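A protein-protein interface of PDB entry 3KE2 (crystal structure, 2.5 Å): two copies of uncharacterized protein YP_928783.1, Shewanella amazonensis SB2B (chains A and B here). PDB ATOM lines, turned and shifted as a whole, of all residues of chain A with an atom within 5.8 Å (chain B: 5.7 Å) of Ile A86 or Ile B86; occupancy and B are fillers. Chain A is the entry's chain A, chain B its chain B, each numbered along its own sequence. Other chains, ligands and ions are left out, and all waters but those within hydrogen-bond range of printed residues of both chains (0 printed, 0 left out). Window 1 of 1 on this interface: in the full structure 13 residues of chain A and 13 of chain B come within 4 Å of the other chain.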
ATOM      1  N   PHE A  19     -22.668  19.536  33.688  1.00  0.00           N
ATOM      2  CA  PHE A  19     -22.365  20.596  32.728  1.00  0.00           C
ATOM      3  C   PHE A  19     -21.901  19.993  31.407  1.00  0.00           C
ATOM      4  O   PHE A  19     -22.382  20.358  30.351  1.00  0.00           O
ATOM      5  CB  PHE A  19     -21.306  21.549  33.332  1.00  0.00           C
ATOM      6  CG  PHE A  19     -20.808  22.625  32.387  1.00  0.00           C
ATOM      7  CD1 PHE A  19     -21.542  23.780  32.179  1.00  0.00           C
ATOM      8  CD2 PHE A  19     -19.570  22.492  31.743  1.00  0.00           C
ATOM      9  CE1 PHE A  19     -21.084  24.753  31.313  1.00  0.00           C
ATOM     10  CE2 PHE A  19     -19.110  23.465  30.892  1.00  0.00           C
ATOM     11  CZ  PHE A  19     -19.867  24.593  30.670  1.00  0.00           C
ATOM     12  N   LEU A  23     -23.269  20.137  27.398  1.00  0.00           N
ATOM     13  CA  LEU A  23     -22.455  20.465  26.208  1.00  0.00           C
ATOM     14  C   LEU A  23     -22.419  19.351  25.192  1.00  0.00           C
ATOM     15  O   LEU A  23     -22.360  19.603  23.978  1.00  0.00           O
ATOM     16  CB  LEU A  23     -21.019  20.848  26.574  1.00  0.00           C
ATOM     17  CG  LEU A  23     -20.690  22.308  26.851  1.00  0.00           C
ATOM     18  CD1 LEU A  23     -21.740  23.008  27.626  1.00  0.00           C
ATOM     19  CD2 LEU A  23     -19.340  22.339  27.580  1.00  0.00           C
ATOM     20  N   ILE A  60     -27.209  27.864  31.175  1.00  0.00           N
ATOM     21  CA  ILE A  60     -25.850  28.169  30.739  1.00  0.00           C
ATOM     22  C   ILE A  60     -25.831  28.973  29.440  1.00  0.00           C
ATOM     23  O   ILE A  60     -24.809  29.059  28.783  1.00  0.00           O
ATOM     24  CB  ILE A  60     -24.984  26.871  30.639  1.00  0.00           C
ATOM     25  CG1 ILE A  60     -25.479  25.898  29.559  1.00  0.00           C
ATOM     26  CG2 ILE A  60     -24.940  26.186  32.037  1.00  0.00           C
ATOM     27  CD1 ILE A  60     -24.449  24.772  29.186  1.00  0.00           C
ATOM     28  N   GLY A  61     -26.966  29.568  29.080  1.00  0.00           N
ATOM     29  CA  GLY A  61     -27.057  30.418  27.872  1.00  0.00           C
ATOM     30  C   GLY A  61     -27.221  29.783  26.498  1.00  0.00           C
ATOM     31  O   GLY A  61     -27.040  30.456  25.486  1.00  0.00           O
ATOM     32  N   ILE A  62     -27.511  28.488  26.456  1.00  0.00           N
ATOM     33  CA  ILE A  62     -27.737  27.794  25.188  1.00  0.00           C
ATOM     34  C   ILE A  62     -29.248  27.816  24.952  1.00  0.00           C
ATOM     35  O   ILE A  62     -30.024  27.265  25.758  1.00  0.00           O
ATOM     36  CB  ILE A  62     -27.212  26.350  25.186  1.00  0.00           C
ATOM     37  CG1 ILE A  62     -25.704  26.330  25.451  1.00  0.00           C
ATOM     38  CG2 ILE A  62     -27.489  25.692  23.872  1.00  0.00           C
ATOM     39  CD1 ILE A  62     -25.059  24.919  25.500  1.00  0.00           C
ATOM     40  N   TRP A  83     -25.572  29.465  20.852  1.00  0.00           N
ATOM     41  CA  TRP A  83     -24.709  28.850  21.856  1.00  0.00           C
ATOM     42  C   TRP A  83     -24.401  29.825  22.968  1.00  0.00           C
ATOM     43  O   TRP A  83     -23.967  29.422  24.046  1.00  0.00           O
ATOM     44  CB  TRP A  83     -23.395  28.386  21.254  1.00  0.00           C
ATOM     45  CG  TRP A  83     -23.514  27.149  20.486  1.00  0.00           C
ATOM     46  CD1 TRP A  83     -23.859  27.029  19.184  1.00  0.00           C
ATOM     47  CD2 TRP A  83     -23.259  25.824  20.966  1.00  0.00           C
ATOM     48  NE1 TRP A  83     -23.845  25.710  18.821  1.00  0.00           N
ATOM     49  CE2 TRP A  83     -23.490  24.947  19.897  1.00  0.00           C
ATOM     50  CE3 TRP A  83     -22.857  25.297  22.202  1.00  0.00           C
ATOM     51  CZ2 TRP A  83     -23.326  23.570  20.010  1.00  0.00           C
ATOM     52  CZ3 TRP A  83     -22.693  23.913  22.318  1.00  0.00           C
ATOM     53  CH2 TRP A  83     -22.935  23.069  21.225  1.00  0.00           C
ATOM     54  N   GLY A  84     -24.602  31.109  22.689  1.00  0.00           N
ATOM     55  CA  GLY A  84     -24.329  32.156  23.647  1.00  0.00           C
ATOM     56  C   GLY A  84     -22.898  32.143  24.156  1.00  0.00           C
ATOM     57  O   GLY A  84     -21.958  32.166  23.372  1.00  0.00           O
ATOM     58  N   PRO A  85     -22.724  32.054  25.475  1.00  0.00           N
ATOM     59  CA  PRO A  85     -21.385  32.120  26.032  1.00  0.00           C
ATOM     60  C   PRO A  85     -20.566  30.847  25.857  1.00  0.00           C
ATOM     61  O   PRO A  85     -19.382  30.836  26.243  1.00  0.00           O
ATOM     62  CB  PRO A  85     -21.663  32.330  27.525  1.00  0.00           C
ATOM     63  CG  PRO A  85     -22.873  31.547  27.770  1.00  0.00           C
ATOM     64  CD  PRO A  85     -23.717  31.708  26.512  1.00  0.00           C
ATOM     65  N   ILE A  86     -21.181  29.798  25.308  1.00  0.00           N
ATOM     66  CA  ILE A  86     -20.524  28.513  25.131  1.00  0.00           C
ATOM     67  C   ILE A  86     -19.872  28.392  23.764  1.00  0.00           C
ATOM     68  O   ILE A  86     -20.447  28.731  22.717  1.00  0.00           O
ATOM     69  CB  ILE A  86     -21.520  27.350  25.296  1.00  0.00           C
ATOM     70  CG1 ILE A  86     -22.243  27.450  26.644  1.00  0.00           C
ATOM     71  CG2 ILE A  86     -20.824  26.010  25.173  1.00  0.00           C
ATOM     72  CD1 ILE A  86     -21.364  27.539  27.806  1.00  0.00           C
ATOM     73  N   SER A  87     -18.653  27.894  23.787  1.00  0.00           N
ATOM     74  CA  SER A  87     -17.892  27.695  22.599  1.00  0.00           C
ATOM     75  C   SER A  87     -18.178  26.300  22.070  1.00  0.00           C
ATOM     76  O   SER A  87     -17.814  25.313  22.683  1.00  0.00           O
ATOM     77  CB  SER A  87     -16.413  27.848  22.915  1.00  0.00           C
ATOM     78  OG  SER A  87     -15.620  27.626  21.763  1.00  0.00           O
ATOM     79  N   SER A  88     -18.846  26.226  20.931  1.00  0.00           N
ATOM     80  CA  SER A  88     -19.145  24.948  20.313  1.00  0.00           C
ATOM     81  C   SER A  88     -17.863  24.233  19.866  1.00  0.00           C
ATOM     82  O   SER A  88     -17.762  23.020  19.980  1.00  0.00           O
ATOM     83  CB  SER A  88     -20.066  25.151  19.117  1.00  0.00           C
ATOM     84  OG  SER A  88     -19.403  25.888  18.119  1.00  0.00           O
ATOM     85  N   PHE B  19     -24.400  31.295  37.370  1.00  0.00           N
ATOM     86  CA  PHE B  19     -23.534  31.071  36.195  1.00  0.00           C
ATOM     87  C   PHE B  19     -22.971  32.370  35.651  1.00  0.00           C
ATOM     88  O   PHE B  19     -21.785  32.483  35.391  1.00  0.00           O
ATOM     89  CB  PHE B  19     -24.322  30.307  35.102  1.00  0.00           C
ATOM     90  CG  PHE B  19     -23.546  30.063  33.835  1.00  0.00           C
ATOM     91  CD1 PHE B  19     -22.685  29.001  33.733  1.00  0.00           C
ATOM     92  CD2 PHE B  19     -23.714  30.883  32.734  1.00  0.00           C
ATOM     93  CE1 PHE B  19     -21.988  28.775  32.580  1.00  0.00           C
ATOM     94  CE2 PHE B  19     -23.014  30.664  31.580  1.00  0.00           C
ATOM     95  CZ  PHE B  19     -22.155  29.607  31.500  1.00  0.00           C
ATOM     96  N   LEU B  23     -18.947  33.979  35.135  1.00  0.00           N
ATOM     97  CA  LEU B  23     -18.437  34.588  33.894  1.00  0.00           C
ATOM     98  C   LEU B  23     -18.085  36.044  34.095  1.00  0.00           C
ATOM     99  O   LEU B  23     -17.140  36.532  33.472  1.00  0.00           O
ATOM    100  CB  LEU B  23     -19.412  34.440  32.713  1.00  0.00           C
ATOM    101  CG  LEU B  23     -19.417  33.108  31.951  1.00  0.00           C
ATOM    102  CD1 LEU B  23     -19.666  31.895  32.842  1.00  0.00           C
ATOM    103  CD2 LEU B  23     -20.468  33.183  30.841  1.00  0.00           C
ATOM    104  N   ILE B  60     -17.318  24.694  35.315  1.00  0.00           N
ATOM    105  CA  ILE B  60     -17.749  25.141  34.005  1.00  0.00           C
ATOM    106  C   ILE B  60     -16.521  25.267  33.064  1.00  0.00           C
ATOM    107  O   ILE B  60     -16.579  25.943  32.037  1.00  0.00           O
ATOM    108  CB  ILE B  60     -18.614  26.444  34.081  1.00  0.00           C
ATOM    109  CG1 ILE B  60     -17.785  27.644  34.545  1.00  0.00           C
ATOM    110  CG2 ILE B  60     -19.848  26.221  34.982  1.00  0.00           C
ATOM    111  CD1 ILE B  60     -18.584  28.937  34.583  1.00  0.00           C
ATOM    112  N   GLY B  61     -15.419  24.606  33.423  1.00  0.00           N
ATOM    113  CA  GLY B  61     -14.201  24.590  32.594  1.00  0.00           C
ATOM    114  C   GLY B  61     -13.270  25.796  32.597  1.00  0.00           C
ATOM    115  O   GLY B  61     -12.412  25.909  31.714  1.00  0.00           O
ATOM    116  N   ILE B  62     -13.437  26.715  33.542  1.00  0.00           N
ATOM    117  CA  ILE B  62     -12.552  27.851  33.615  1.00  0.00           C
ATOM    118  C   ILE B  62     -11.482  27.513  34.637  1.00  0.00           C
ATOM    119  O   ILE B  62     -11.790  27.257  35.791  1.00  0.00           O
ATOM    120  CB  ILE B  62     -13.271  29.141  34.005  1.00  0.00           C
ATOM    121  CG1 ILE B  62     -14.337  29.494  32.968  1.00  0.00           C
ATOM    122  CG2 ILE B  62     -12.272  30.283  34.125  1.00  0.00           C
ATOM    123  CD1 ILE B  62     -15.189  30.698  33.361  1.00  0.00           C
ATOM    124  N   TRP B  83     -10.088  29.640  29.481  1.00  0.00           N
ATOM    125  CA  TRP B  83     -11.537  29.777  29.565  1.00  0.00           C
ATOM    126  C   TRP B  83     -12.243  28.487  29.168  1.00  0.00           C
ATOM    127  O   TRP B  83     -13.444  28.329  29.397  1.00  0.00           O
ATOM    128  CB  TRP B  83     -12.019  30.892  28.650  1.00  0.00           C
ATOM    129  CG  TRP B  83     -11.747  32.239  29.125  1.00  0.00           C
ATOM    130  CD1 TRP B  83     -10.589  32.932  29.001  1.00  0.00           C
ATOM    131  CD2 TRP B  83     -12.676  33.100  29.774  1.00  0.00           C
ATOM    132  NE1 TRP B  83     -10.732  34.193  29.546  1.00  0.00           N
ATOM    133  CE2 TRP B  83     -12.008  34.313  30.040  1.00  0.00           C
ATOM    134  CE3 TRP B  83     -14.002  32.963  30.171  1.00  0.00           C
ATOM    135  CZ2 TRP B  83     -12.640  35.394  30.674  1.00  0.00           C
ATOM    136  CZ3 TRP B  83     -14.630  34.036  30.793  1.00  0.00           C
ATOM    137  CH2 TRP B  83     -13.949  35.234  31.043  1.00  0.00           C
ATOM    138  N   GLY B  84     -11.503  27.574  28.550  1.00  0.00           N
ATOM    139  CA  GLY B  84     -12.063  26.311  28.111  1.00  0.00           C
ATOM    140  C   GLY B  84     -13.277  26.511  27.216  1.00  0.00           C
ATOM    141  O   GLY B  84     -13.223  27.254  26.235  1.00  0.00           O
ATOM    142  N   PRO B  85     -14.395  25.905  27.583  1.00  0.00           N
ATOM    143  CA  PRO B  85     -15.589  25.996  26.779  1.00  0.00           C
ATOM    144  C   PRO B  85     -16.336  27.331  26.884  1.00  0.00           C
ATOM    145  O   PRO B  85     -17.361  27.495  26.230  1.00  0.00           O
ATOM    146  CB  PRO B  85     -16.468  24.877  27.358  1.00  0.00           C
ATOM    147  CG  PRO B  85     -16.088  24.797  28.758  1.00  0.00           C
ATOM    148  CD  PRO B  85     -14.664  25.264  28.880  1.00  0.00           C
ATOM    149  N   ILE B  86     -15.867  28.251  27.714  1.00  0.00           N
ATOM    150  CA  ILE B  86     -16.539  29.530  27.861  1.00  0.00           C
ATOM    151  C   ILE B  86     -15.921  30.542  26.904  1.00  0.00           C
ATOM    152  O   ILE B  86     -14.696  30.641  26.786  1.00  0.00           O
ATOM    153  CB  ILE B  86     -16.460  30.035  29.324  1.00  0.00           C
ATOM    154  CG1 ILE B  86     -17.089  29.012  30.265  1.00  0.00           C
ATOM    155  CG2 ILE B  86     -17.132  31.383  29.480  1.00  0.00           C
ATOM    156  CD1 ILE B  86     -18.510  28.611  29.923  1.00  0.00           C
ATOM    157  N   SER B  87     -16.768  31.299  26.223  1.00  0.00           N
ATOM    158  CA  SER B  87     -16.296  32.293  25.288  1.00  0.00           C
ATOM    159  C   SER B  87     -16.070  33.604  26.012  1.00  0.00           C
ATOM    160  O   SER B  87     -17.022  34.258  26.446  1.00  0.00           O
ATOM    161  CB  SER B  87     -17.305  32.486  24.157  1.00  0.00           C
ATOM    162  OG  SER B  87     -16.852  33.497  23.264  1.00  0.00           O
ATOM    163  N   SER B  88     -14.807  33.996  26.148  1.00  0.00           N
ATOM    164  CA  SER B  88     -14.485  35.249  26.796  1.00  0.00           C
ATOM    165  C   SER B  88     -14.953  36.439  25.936  1.00  0.00           C
ATOM    166  O   SER B  88     -15.161  37.546  26.437  1.00  0.00           O
ATOM    167  CB  SER B  88     -12.999  35.331  27.039  1.00  0.00           C
ATOM    168  OG  SER B  88     -12.303  35.330  25.822  1.00  0.00           O
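Phe A19 touches Ile B60, and with the chains exchanged Ile A60 touches Phe B19. Leu A23 touches Pro B85, and with the chains exchanged Pro A85 touches Leu B23. Pro A85 touches its own counterpart, Pro B85. Pro A85 touches Ser B87, and with the chains exchanged Ser A87 touches Pro B85. Positions printed for both chains: 19, 23, 60, 61, 62, 83, 84, 85, 86, 87 and 88.
Hydrophobic or aromatic side chains of chain A that line the printed part of chain B: Phe A19, Leu A23, Ile A60, Pro A85 and Ile A86. Among the printed residues, 12 pairs touch across the chains.
The backbone NH (N) of Ser B87 is in hydrogen-bond range of the backbone carbonyl oxygen (O) of Pro A85 (2.7 Å). The backbone NH of Ser A87 lies within hydrogen-bond range of the backbone carbonyl oxygen of Pro B85.
Ile A62 touches none of the printed residues of chain B. Of the printed residues of chain B, Pro A85 touches Phe B19 (3.9 Å), Leu B23 (3.6 Å), Pro B85 (3.9 Å), Ile B86 (3.5 Å) and Ser B87 (2.7 Å). Ile A86 touches just these residues of chain B: Pro B85 and Ile B86. Printed residues of chain A within 4 Å of Phe B19: Ile A60 and Pro A85. Of the printed residues of chain A, Leu B23 touches Pro A85. Ile B86 touches just these residues of chain A: Pro A85 (3.5 Å) and Ile A86 (3.7 Å). Of the printed residues of chain A, Ser B87 touches Pro A85. The nearest residue of chain B that does not touch Ile A86 is Phe B19 (4.3 Å). The nearest printed residue of chain A that does not touch Ile B60 is Ile A60 (5.9 Å).
Ile B60 touches Phe A19 (O to CE2, 3.7 Å). Phe A19 touches Pro B85 (CE2 to CG, 3.9 Å). Leu A23 touches Pro B85 (CD2 to CB, 3.8 Å). Ile A60 touches Phe B19. CE2 of Phe B19 touches CG of Pro A85 (3.9 Å). CD2 of Leu B23 touches CB of Pro A85, at 3.6 Å. Pro A85 touches Pro B85. Pro A85 touches Ile B86. Ile A86 touches Pro B85. Ile A86 touches Ile B86 (CD1 to CD1, 3.7 Å).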
